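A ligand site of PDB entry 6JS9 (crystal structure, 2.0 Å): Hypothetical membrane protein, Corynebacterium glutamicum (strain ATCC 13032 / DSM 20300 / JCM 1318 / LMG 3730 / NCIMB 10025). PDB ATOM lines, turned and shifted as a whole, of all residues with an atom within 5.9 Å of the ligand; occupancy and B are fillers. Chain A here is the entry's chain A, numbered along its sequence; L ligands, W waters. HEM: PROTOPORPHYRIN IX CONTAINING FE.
NE2 of His 77 lies close to NC of the ligand (3.2 Å).
CG1 of Val 29 touches C2D of the ligand, at 3.9 Å.
Ile 84 touches the ligand (O to CBB, 3.5 Å).
CD1 of Leu 85 touches C2B of the ligand, at 3.4 Å.
Arg 110 touches the ligand (O to CBB, 3.3 Å).
Glu 111 touches the ligand.
Phe 112 touches the ligand (CD1 to C4B, 3.5 Å).
O of Gly 114 touches CMC of the ligand (3.6 Å).
Thr 115 touches the ligand.
Thr 116 touches the ligand (N to CBC, 3.4 Å).
Tyr 117 touches the ligand (CE1 to CBC, 3.6 Å).
O of Phe 163 touches CHB of the ligand, at 3.6 Å.
Gly 164 touches the ligand (N to CMB, 3.9 Å).
Phe 166 touches the ligand (CD1 to C4A, 3.3 Å).
Hydrophobic or aromatic side chains that line the ligand: Phe 21, Tyr 24, Val 29, His 77, Ile 84, Leu 85, Phe 112, Tyr 117, Phe 166 and Tyr 167.
18 residues have an atom within 4 Å of the ligand: Ser 20, Phe 21, Tyr 24, Val 29, His 77, Ile 84, Leu 85, Arg 110, Glu 111, Phe 112, Gly 114, Thr 115, Thr 116, Tyr 117, Phe 163, Gly 164, Phe 166 and Tyr 167.
The nearest printed residue that does not touch the ligand is Arg 18 (4.1 Å).
The side-chain hydroxyl of Tyr 24 lies close to a ring nitrogen (NE2) of His 77.
OG of Ser 20 sits at hydrogen-bond distance from NE of Arg 18, at 2.8 Å.
A ring nitrogen (ND1) of His 77 is in hydrogen-bond range of the side-chain hydroxyl of Tyr 117, at 2.7 Å.
The backbone carbonyl oxygen (O) of Asp 86 sits at hydrogen-bond distance from the backbone NH (N) of Arg 110.
The backbone NH of Ile 84 is in hydrogen-bond range of the backbone carbonyl oxygen of His 77 (2.9 Å).
Water W4 lies within hydrogen-bond range of an oxygen (O1D) of the ligand (2.6 Å) and the backbone NH of Val 29 (2.9 Å).
Water W3 lies within hydrogen-bond range of the backbone carbonyl oxygen of Arg 110, the backbone NH of Asp 86 and the side-chain hydroxyl of Thr 87.
The backbone NH (N) of Phe 21 sits at hydrogen-bond distance from an oxygen (O1A) of the ligand.
An iron atom (FE) of the ligand is bound by the side-chain hydroxyl (OH) of Tyr 24 (2.3 Å).
O1A of the ligand lies within hydrogen-bond range of OG of Ser 20 (2.5 Å).
The side-chain hydroxyl (OH) of Tyr 167 lies within hydrogen-bond range of an oxygen (O1A) of the ligand.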
ATOM      1  N   PHE A  17     -29.500  25.445 -26.060  1.00  0.00           N
ATOM      2  CA  PHE A  17     -28.371  24.595 -26.464  1.00  0.00           C
ATOM      3  C   PHE A  17     -28.238  24.536 -27.985  1.00  0.00           C
ATOM      4  O   PHE A  17     -27.358  25.189 -28.560  1.00  0.00           O
ATOM      5  CB  PHE A  17     -28.496  23.191 -25.870  1.00  0.00           C
ATOM      6  CG  PHE A  17     -27.396  22.243 -26.281  1.00  0.00           C
ATOM      7  CD1 PHE A  17     -26.067  22.547 -26.015  1.00  0.00           C
ATOM      8  CD2 PHE A  17     -27.693  21.044 -26.918  1.00  0.00           C
ATOM      9  CE1 PHE A  17     -25.036  21.674 -26.391  1.00  0.00           C
ATOM     10  CE2 PHE A  17     -26.669  20.159 -27.284  1.00  0.00           C
ATOM     11  CZ  PHE A  17     -25.327  20.491 -27.015  1.00  0.00           C
ATOM     12  N   ARG A  18     -29.099  23.773 -28.653  1.00  0.00           N
ATOM     13  CA  ARG A  18     -29.010  23.621 -30.107  1.00  0.00           C
ATOM     14  C   ARG A  18     -30.316  23.080 -30.656  1.00  0.00           C
ATOM     15  O   ARG A  18     -30.752  21.991 -30.259  1.00  0.00           O
ATOM     16  CB  ARG A  18     -27.856  22.691 -30.488  1.00  0.00           C
ATOM     17  CG  ARG A  18     -27.857  22.368 -31.959  1.00  0.00           C
ATOM     18  CD  ARG A  18     -26.476  22.147 -32.495  1.00  0.00           C
ATOM     19  NE  ARG A  18     -26.562  21.519 -33.803  1.00  0.00           N
ATOM     20  CZ  ARG A  18     -25.552  21.375 -34.636  1.00  0.00           C
ATOM     21  NH1 ARG A  18     -24.353  21.839 -34.313  1.00  0.00           N
ATOM     22  NH2 ARG A  18     -25.744  20.771 -35.801  1.00  0.00           N
ATOM     23  N   SER A  20     -31.309  21.669 -33.366  1.00  0.00           N
ATOM     24  CA  SER A  20     -31.320  20.326 -33.957  1.00  0.00           C
ATOM     25  C   SER A  20     -31.295  19.247 -32.887  1.00  0.00           C
ATOM     26  O   SER A  20     -31.855  18.160 -33.094  1.00  0.00           O
ATOM     27  CB  SER A  20     -30.147  20.150 -34.923  1.00  0.00           C
ATOM     28  OG  SER A  20     -28.918  20.041 -34.200  1.00  0.00           O
ATOM     29  N   PHE A  21     -30.645  19.507 -31.760  1.00  0.00           N
ATOM     30  CA  PHE A  21     -30.690  18.545 -30.665  1.00  0.00           C
ATOM     31  C   PHE A  21     -32.077  18.469 -30.046  1.00  0.00           C
ATOM     32  O   PHE A  21     -32.586  17.372 -29.791  1.00  0.00           O
ATOM     33  CB  PHE A  21     -29.637  18.881 -29.614  1.00  0.00           C
ATOM     34  CG  PHE A  21     -29.519  17.833 -28.557  1.00  0.00           C
ATOM     35  CD1 PHE A  21     -29.031  16.566 -28.875  1.00  0.00           C
ATOM     36  CD2 PHE A  21     -29.890  18.089 -27.248  1.00  0.00           C
ATOM     37  CE1 PHE A  21     -28.910  15.599 -27.905  1.00  0.00           C
ATOM     38  CE2 PHE A  21     -29.779  17.114 -26.277  1.00  0.00           C
ATOM     39  CZ  PHE A  21     -29.286  15.870 -26.613  1.00  0.00           C
ATOM     40  N   TYR A  24     -34.063  16.553 -32.484  1.00  0.00           N
ATOM     41  CA  TYR A  24     -33.639  15.164 -32.375  1.00  0.00           C
ATOM     42  C   TYR A  24     -34.323  14.469 -31.200  1.00  0.00           C
ATOM     43  O   TYR A  24     -34.880  13.372 -31.367  1.00  0.00           O
ATOM     44  CB  TYR A  24     -32.107  15.134 -32.263  1.00  0.00           C
ATOM     45  CG  TYR A  24     -31.556  13.837 -31.734  1.00  0.00           C
ATOM     46  CD1 TYR A  24     -31.592  12.675 -32.507  1.00  0.00           C
ATOM     47  CD2 TYR A  24     -30.981  13.777 -30.473  1.00  0.00           C
ATOM     48  CE1 TYR A  24     -31.072  11.497 -32.022  1.00  0.00           C
ATOM     49  CE2 TYR A  24     -30.456  12.605 -29.977  1.00  0.00           C
ATOM     50  CZ  TYR A  24     -30.515  11.468 -30.757  1.00  0.00           C
ATOM     51  OH  TYR A  24     -30.010  10.288 -30.256  1.00  0.00           O
ATOM     52  N   GLY A  28     -37.342  13.505 -33.425  1.00  0.00           N
ATOM     53  CA  GLY A  28     -36.483  12.620 -34.182  1.00  0.00           C
ATOM     54  C   GLY A  28     -36.337  11.252 -33.553  1.00  0.00           C
ATOM     55  O   GLY A  28     -37.169  10.801 -32.763  1.00  0.00           O
ATOM     56  N   VAL A  29     -35.218  10.591 -33.868  1.00  0.00           N
ATOM     57  CA  VAL A  29     -35.062   9.170 -33.553  1.00  0.00           C
ATOM     58  C   VAL A  29     -34.940   8.909 -32.047  1.00  0.00           C
ATOM     59  O   VAL A  29     -35.227   7.796 -31.589  1.00  0.00           O
ATOM     60  CB  VAL A  29     -33.873   8.603 -34.360  1.00  0.00           C
ATOM     61  CG1 VAL A  29     -32.530   9.118 -33.853  1.00  0.00           C
ATOM     62  CG2 VAL A  29     -33.906   7.074 -34.403  1.00  0.00           C
ATOM     63  N   HIS A  77     -34.189   7.600 -26.308  1.00  0.00           N
ATOM     64  CA  HIS A  77     -33.845   6.199 -26.591  1.00  0.00           C
ATOM     65  C   HIS A  77     -34.263   5.277 -25.442  1.00  0.00           C
ATOM     66  O   HIS A  77     -33.444   4.671 -24.748  1.00  0.00           O
ATOM     67  CB  HIS A  77     -32.340   6.081 -26.889  1.00  0.00           C
ATOM     68  CG  HIS A  77     -31.930   6.735 -28.165  1.00  0.00           C
ATOM     69  ND1 HIS A  77     -32.418   6.349 -29.385  1.00  0.00           N
ATOM     70  CD2 HIS A  77     -31.079   7.761 -28.407  1.00  0.00           C
ATOM     71  CE1 HIS A  77     -31.902   7.107 -30.329  1.00  0.00           C
ATOM     72  NE2 HIS A  77     -31.083   7.971 -29.761  1.00  0.00           N
ATOM     73  N   ILE A  84     -31.529   5.388 -22.677  1.00  0.00           N
ATOM     74  CA  ILE A  84     -30.108   5.267 -23.001  1.00  0.00           C
ATOM     75  C   ILE A  84     -29.449   6.643 -23.121  1.00  0.00           C
ATOM     76  O   ILE A  84     -28.287   6.808 -22.737  1.00  0.00           O
ATOM     77  CB  ILE A  84     -29.911   4.413 -24.262  1.00  0.00           C
ATOM     78  CG1 ILE A  84     -30.401   2.990 -23.996  1.00  0.00           C
ATOM     79  CG2 ILE A  84     -28.454   4.379 -24.674  1.00  0.00           C
ATOM     80  CD1 ILE A  84     -30.159   2.042 -25.146  1.00  0.00           C
ATOM     81  N   LEU A  85     -30.168   7.647 -23.629  1.00  0.00           N
ATOM     82  CA  LEU A  85     -29.729   9.036 -23.536  1.00  0.00           C
ATOM     83  C   LEU A  85     -30.422   9.645 -22.311  1.00  0.00           C
ATOM     84  O   LEU A  85     -31.650   9.816 -22.315  1.00  0.00           O
ATOM     85  CB  LEU A  85     -30.055   9.819 -24.803  1.00  0.00           C
ATOM     86  CG  LEU A  85     -29.418  11.231 -24.927  1.00  0.00           C
ATOM     87  CD1 LEU A  85     -29.326  11.652 -26.398  1.00  0.00           C
ATOM     88  CD2 LEU A  85     -30.181  12.303 -24.140  1.00  0.00           C
ATOM     89  N   ASP A  86     -29.634   9.983 -21.287  1.00  0.00           N
ATOM     90  CA  ASP A  86     -30.175  10.580 -20.054  1.00  0.00           C
ATOM     91  C   ASP A  86     -29.146  11.612 -19.578  1.00  0.00           C
ATOM     92  O   ASP A  86     -28.235  11.279 -18.818  1.00  0.00           O
ATOM     93  CB  ASP A  86     -30.447   9.506 -19.009  1.00  0.00           C
ATOM     94  CG  ASP A  86     -31.171  10.034 -17.774  1.00  0.00           C
ATOM     95  OD1 ASP A  86     -31.097  11.241 -17.484  1.00  0.00           O
ATOM     96  OD2 ASP A  86     -31.837   9.231 -17.086  1.00  0.00           O
ATOM     97  N   THR A  87     -29.321  12.875 -20.007  1.00  0.00           N
ATOM     98  CA  THR A  87     -28.403  13.967 -19.727  1.00  0.00           C
ATOM     99  C   THR A  87     -29.135  15.082 -19.005  1.00  0.00           C
ATOM    100  O   THR A  87     -30.166  15.561 -19.473  1.00  0.00           O
ATOM    101  CB  THR A  87     -27.783  14.539 -21.001  1.00  0.00           C
ATOM    102  OG1 THR A  87     -27.054  13.520 -21.685  1.00  0.00           O
ATOM    103  CG2 THR A  87     -26.839  15.718 -20.663  1.00  0.00           C
ATOM    104  N   ARG A 110     -25.459   9.884 -19.010  1.00  0.00           N
ATOM    105  CA  ARG A 110     -25.015   8.547 -19.408  1.00  0.00           C
ATOM    106  C   ARG A 110     -23.955   8.663 -20.493  1.00  0.00           C
ATOM    107  O   ARG A 110     -24.082   9.455 -21.422  1.00  0.00           O
ATOM    108  CB  ARG A 110     -26.187   7.715 -19.899  1.00  0.00           C
ATOM    109  CG  ARG A 110     -27.126   7.265 -18.785  1.00  0.00           C
ATOM    110  CD  ARG A 110     -28.105   6.228 -19.269  1.00  0.00           C
ATOM    111  NE  ARG A 110     -29.183   6.053 -18.315  1.00  0.00           N
ATOM    112  CZ  ARG A 110     -29.129   5.207 -17.288  1.00  0.00           C
ATOM    113  NH1 ARG A 110     -30.166   5.097 -16.462  1.00  0.00           N
ATOM    114  NH2 ARG A 110     -28.043   4.474 -17.096  1.00  0.00           N
ATOM    115  N   GLU A 111     -22.882   7.887 -20.331  1.00  0.00           N
ATOM    116  CA  GLU A 111     -21.891   7.736 -21.390  1.00  0.00           C
ATOM    117  C   GLU A 111     -22.531   7.152 -22.644  1.00  0.00           C
ATOM    118  O   GLU A 111     -23.381   6.256 -22.564  1.00  0.00           O
ATOM    119  CB  GLU A 111     -20.759   6.825 -20.902  1.00  0.00           C
ATOM    120  CG  GLU A 111     -19.589   6.697 -21.853  1.00  0.00           C
ATOM    121  CD  GLU A 111     -18.553   5.688 -21.380  1.00  0.00           C
ATOM    122  OE1 GLU A 111     -18.874   4.871 -20.477  1.00  0.00           O
ATOM    123  OE2 GLU A 111     -17.419   5.725 -21.900  1.00  0.00           O
ATOM    124  N   PHE A 112     -22.120   7.655 -23.809  1.00  0.00           N
ATOM    125  CA  PHE A 112     -22.581   7.100 -25.075  1.00  0.00           C
ATOM    126  C   PHE A 112     -21.786   5.826 -25.370  1.00  0.00           C
ATOM    127  O   PHE A 112     -20.553   5.852 -25.412  1.00  0.00           O
ATOM    128  CB  PHE A 112     -22.393   8.110 -26.195  1.00  0.00           C
ATOM    129  CG  PHE A 112     -22.603   7.522 -27.557  1.00  0.00           C
ATOM    130  CD1 PHE A 112     -23.867   7.175 -27.989  1.00  0.00           C
ATOM    131  CD2 PHE A 112     -21.527   7.278 -28.398  1.00  0.00           C
ATOM    132  CE1 PHE A 112     -24.063   6.609 -29.230  1.00  0.00           C
ATOM    133  CE2 PHE A 112     -21.725   6.725 -29.645  1.00  0.00           C
ATOM    134  CZ  PHE A 112     -22.992   6.395 -30.060  1.00  0.00           C
ATOM    135  N   LYS A 113     -22.488   4.708 -25.580  1.00  0.00           N
ATOM    136  CA  LYS A 113     -21.818   3.422 -25.747  1.00  0.00           C
ATOM    137  C   LYS A 113     -21.846   2.907 -27.175  1.00  0.00           C
ATOM    138  O   LYS A 113     -21.223   1.880 -27.451  1.00  0.00           O
ATOM    139  CB  LYS A 113     -22.449   2.356 -24.838  1.00  0.00           C
ATOM    140  CG  LYS A 113     -22.403   2.702 -23.365  1.00  0.00           C
ATOM    141  CD  LYS A 113     -20.976   2.856 -22.869  1.00  0.00           C
ATOM    142  CE  LYS A 113     -20.239   1.524 -22.788  1.00  0.00           C
ATOM    143  NZ  LYS A 113     -20.854   0.582 -21.795  1.00  0.00           N
ATOM    144  N   GLY A 114     -22.529   3.587 -28.093  1.00  0.00           N
ATOM    145  CA  GLY A 114     -22.725   3.074 -29.429  1.00  0.00           C
ATOM    146  C   GLY A 114     -24.175   3.186 -29.853  1.00  0.00           C
ATOM    147  O   GLY A 114     -25.050   3.380 -29.009  1.00  0.00           O
ATOM    148  N   THR A 115     -24.444   3.089 -31.156  1.00  0.00           N
ATOM    149  CA  THR A 115     -25.802   3.247 -31.655  1.00  0.00           C
ATOM    150  C   THR A 115     -26.511   1.904 -31.738  1.00  0.00           C
ATOM    151  O   THR A 115     -26.962   1.464 -32.788  1.00  0.00           O
ATOM    152  CB  THR A 115     -25.802   3.955 -33.013  1.00  0.00           C
ATOM    153  OG1 THR A 115     -24.933   3.268 -33.916  1.00  0.00           O
ATOM    154  CG2 THR A 115     -25.351   5.380 -32.860  1.00  0.00           C
ATOM    155  N   THR A 116     -26.592   1.243 -30.579  1.00  0.00           N
ATOM    156  CA  THR A 116     -27.433   0.066 -30.405  1.00  0.00           C
ATOM    157  C   THR A 116     -28.171   0.173 -29.086  1.00  0.00           C
ATOM    158  O   THR A 116     -27.755   0.877 -28.169  1.00  0.00           O
ATOM    159  CB  THR A 116     -26.634  -1.253 -30.419  1.00  0.00           C
ATOM    160  OG1 THR A 116     -26.266  -1.584 -29.073  1.00  0.00           O
ATOM    161  CG2 THR A 116     -25.381  -1.137 -31.265  1.00  0.00           C
ATOM    162  N   TYR A 117     -29.294  -0.543 -28.991  1.00  0.00           N
ATOM    163  CA  TYR A 117     -30.024  -0.629 -27.739  1.00  0.00           C
ATOM    164  C   TYR A 117     -29.619  -1.858 -26.921  1.00  0.00           C
ATOM    165  O   TYR A 117     -30.360  -2.248 -26.003  1.00  0.00           O
ATOM    166  CB  TYR A 117     -31.536  -0.651 -27.993  1.00  0.00           C
ATOM    167  CG  TYR A 117     -32.198   0.684 -28.308  1.00  0.00           C
ATOM    168  CD1 TYR A 117     -31.447   1.834 -28.578  1.00  0.00           C
ATOM    169  CD2 TYR A 117     -33.580   0.789 -28.341  1.00  0.00           C
ATOM    170  CE1 TYR A 117     -32.080   3.048 -28.882  1.00  0.00           C
ATOM    171  CE2 TYR A 117     -34.209   1.979 -28.631  1.00  0.00           C
ATOM    172  CZ  TYR A 117     -33.467   3.107 -28.894  1.00  0.00           C
ATOM    173  OH  TYR A 117     -34.150   4.273 -29.183  1.00  0.00           O
ATOM    174  N   ASP A 119     -26.923  -1.936 -25.105  1.00  0.00           N
ATOM    175  CA  ASP A 119     -25.939  -1.465 -24.146  1.00  0.00           C
ATOM    176  C   ASP A 119     -26.330  -0.054 -23.701  1.00  0.00           C
ATOM    177  O   ASP A 119     -26.949   0.703 -24.455  1.00  0.00           O
ATOM    178  CB  ASP A 119     -24.533  -1.482 -24.731  1.00  0.00           C
ATOM    179  CG  ASP A 119     -23.451  -1.410 -23.677  1.00  0.00           C
ATOM    180  OD1 ASP A 119     -23.772  -1.621 -22.484  1.00  0.00           O
ATOM    181  OD2 ASP A 119     -22.288  -1.146 -24.033  1.00  0.00           O
ATOM    182  N   ALA A 162     -19.044  15.114 -24.357  1.00  0.00           N
ATOM    183  CA  ALA A 162     -20.156  14.909 -23.432  1.00  0.00           C
ATOM    184  C   ALA A 162     -21.462  14.594 -24.158  1.00  0.00           C
ATOM    185  O   ALA A 162     -22.362  14.000 -23.559  1.00  0.00           O
ATOM    186  CB  ALA A 162     -20.336  16.151 -22.561  1.00  0.00           C
ATOM    187  N   PHE A 163     -21.583  14.986 -25.420  1.00  0.00           N
ATOM    188  CA  PHE A 163     -22.774  14.706 -26.187  1.00  0.00           C
ATOM    189  C   PHE A 163     -22.523  13.620 -27.237  1.00  0.00           C
ATOM    190  O   PHE A 163     -22.994  13.708 -28.363  1.00  0.00           O
ATOM    191  CB  PHE A 163     -23.318  15.983 -26.812  1.00  0.00           C
ATOM    192  CG  PHE A 163     -24.087  16.835 -25.832  1.00  0.00           C
ATOM    193  CD1 PHE A 163     -23.421  17.718 -24.986  1.00  0.00           C
ATOM    194  CD2 PHE A 163     -25.467  16.747 -25.745  1.00  0.00           C
ATOM    195  CE1 PHE A 163     -24.118  18.501 -24.061  1.00  0.00           C
ATOM    196  CE2 PHE A 163     -26.182  17.517 -24.840  1.00  0.00           C
ATOM    197  CZ  PHE A 163     -25.506  18.408 -23.995  1.00  0.00           C
ATOM    198  N   GLY A 164     -21.754  12.596 -26.851  1.00  0.00           N
ATOM    199  CA  GLY A 164     -21.624  11.381 -27.631  1.00  0.00           C
ATOM    200  C   GLY A 164     -20.707  11.450 -28.833  1.00  0.00           C
ATOM    201  O   GLY A 164     -20.636  10.469 -29.604  1.00  0.00           O
ATOM    202  N   PHE A 166     -21.090  13.156 -31.499  1.00  0.00           N
ATOM    203  CA  PHE A 166     -21.815  13.360 -32.754  1.00  0.00           C
ATOM    204  C   PHE A 166     -21.510  14.714 -33.370  1.00  0.00           C
ATOM    205  O   PHE A 166     -21.486  14.841 -34.604  1.00  0.00           O
ATOM    206  CB  PHE A 166     -23.322  13.211 -32.508  1.00  0.00           C
ATOM    207  CG  PHE A 166     -23.750  11.802 -32.161  1.00  0.00           C
ATOM    208  CD1 PHE A 166     -23.581  11.303 -30.869  1.00  0.00           C
ATOM    209  CD2 PHE A 166     -24.300  10.964 -33.134  1.00  0.00           C
ATOM    210  CE1 PHE A 166     -23.971   9.999 -30.549  1.00  0.00           C
ATOM    211  CE2 PHE A 166     -24.692   9.672 -32.821  1.00  0.00           C
ATOM    212  CZ  PHE A 166     -24.526   9.176 -31.539  1.00  0.00           C
ATOM    213  N   TYR A 167     -21.293  15.736 -32.546  1.00  0.00           N
ATOM    214  CA  TYR A 167     -20.827  17.031 -33.005  1.00  0.00           C
ATOM    215  C   TYR A 167     -19.302  17.057 -33.040  1.00  0.00           C
ATOM    216  O   TYR A 167     -18.638  16.370 -32.260  1.00  0.00           O
ATOM    217  CB  TYR A 167     -21.314  18.148 -32.083  1.00  0.00           C
ATOM    218  CG  TYR A 167     -22.813  18.261 -31.942  1.00  0.00           C
ATOM    219  CD1 TYR A 167     -23.651  18.275 -33.069  1.00  0.00           C
ATOM    220  CD2 TYR A 167     -23.397  18.342 -30.694  1.00  0.00           C
ATOM    221  CE1 TYR A 167     -25.022  18.390 -32.928  1.00  0.00           C
ATOM    222  CE2 TYR A 167     -24.776  18.446 -30.543  1.00  0.00           C
ATOM    223  CZ  TYR A 167     -25.589  18.476 -31.664  1.00  0.00           C
ATOM    224  OH  TYR A 167     -26.961  18.606 -31.497  1.00  0.00           O
HETATM  225  CHA HEM L   1     -27.756  11.987 -33.433  1.00  0.00           C
HETATM  226  CHB HEM L   1     -26.251  12.172 -28.823  1.00  0.00           C
HETATM  227  CHC HEM L   1     -27.497   7.518 -28.110  1.00  0.00           C
HETATM  228  CHD HEM L   1     -28.572   7.208 -32.840  1.00  0.00           C
HETATM  229  C1A HEM L   1     -27.260  12.459 -32.235  1.00  0.00           C
HETATM  230  C2A HEM L   1     -26.851  13.819 -31.955  1.00  0.00           C
HETATM  231  C3A HEM L   1     -26.433  13.890 -30.678  1.00  0.00           C
HETATM  232  C4A HEM L   1     -26.572  12.554 -30.105  1.00  0.00           C
HETATM  233  CMA HEM L   1     -25.897  15.167 -29.983  1.00  0.00           C
HETATM  234  CAA HEM L   1     -26.902  14.971 -32.963  1.00  0.00           C
HETATM  235  CBA HEM L   1     -28.361  15.410 -33.139  1.00  0.00           C
HETATM  236  CGA HEM L   1     -28.392  16.617 -34.040  1.00  0.00           C
HETATM  237  O1A HEM L   1     -28.225  17.757 -33.516  1.00  0.00           O
HETATM  238  O2A HEM L   1     -28.566  16.419 -35.273  1.00  0.00           O
HETATM  239  C1B HEM L   1     -26.443  10.934 -28.236  1.00  0.00           C
HETATM  240  C2B HEM L   1     -26.080  10.588 -26.871  1.00  0.00           C
HETATM  241  C3B HEM L   1     -26.423   9.303 -26.661  1.00  0.00           C
HETATM  242  C4B HEM L   1     -27.021   8.791 -27.899  1.00  0.00           C
HETATM  243  CMB HEM L   1     -25.423  11.608 -25.895  1.00  0.00           C
HETATM  244  CAB HEM L   1     -26.285   8.400 -25.394  1.00  0.00           C
HETATM  245  CBB HEM L   1     -25.763   8.793 -24.229  1.00  0.00           C
HETATM  246  C1C HEM L   1     -27.888   6.996 -29.336  1.00  0.00           C
HETATM  247  C2C HEM L   1     -28.343   5.649 -29.597  1.00  0.00           C
HETATM  248  C3C HEM L   1     -28.645   5.569 -30.905  1.00  0.00           C
HETATM  249  C4C HEM L   1     -28.401   6.865 -31.505  1.00  0.00           C
HETATM  250  CMC HEM L   1     -28.434   4.578 -28.495  1.00  0.00           C
HETATM  251  CAC HEM L   1     -29.174   4.347 -31.708  1.00  0.00           C
HETATM  252  CBC HEM L   1     -29.379   3.136 -31.187  1.00  0.00           C
HETATM  253  C1D HEM L   1     -28.469   8.466 -33.412  1.00  0.00           C
HETATM  254  C2D HEM L   1     -28.788   8.821 -34.801  1.00  0.00           C
HETATM  255  C3D HEM L   1     -28.553  10.141 -34.963  1.00  0.00           C
HETATM  256  C4D HEM L   1     -28.093  10.665 -33.695  1.00  0.00           C
HETATM  257  CMD HEM L   1     -29.302   7.849 -35.890  1.00  0.00           C
HETATM  258  CAD HEM L   1     -28.761  10.994 -36.240  1.00  0.00           C
HETATM  259  CBD HEM L   1     -30.213  11.468 -36.168  1.00  0.00           C
HETATM  260  CGD HEM L   1     -30.593  12.349 -37.334  1.00  0.00           C
HETATM  261  O1D HEM L   1     -31.816  12.482 -37.580  1.00  0.00           O
HETATM  262  O2D HEM L   1     -29.697  12.914 -38.027  1.00  0.00           O
HETATM  263  NA  HEM L   1     -27.083  11.724 -31.090  1.00  0.00           N
HETATM  264  NB  HEM L   1     -27.008   9.802 -28.826  1.00  0.00           N
HETATM  265  NC  HEM L   1     -27.952   7.704 -30.518  1.00  0.00           N
HETATM  266  ND  HEM L   1     -28.062   9.632 -32.789  1.00  0.00           N
HETATM  267 FE   HEM L   1     -27.819   9.804 -30.722  1.00  0.00          FE
HETATM  268  O   HOH W   1     -27.866  14.223 -36.451  1.00  0.00           O
HETATM  269  O   HOH W   2     -33.378  14.713 -38.501  1.00  0.00           O
HETATM  270  O   HOH W   3     -26.776  10.547 -21.804  1.00  0.00           O
HETATM  271  O   HOH W   4     -33.602  12.158 -35.652  1.00  0.00           O
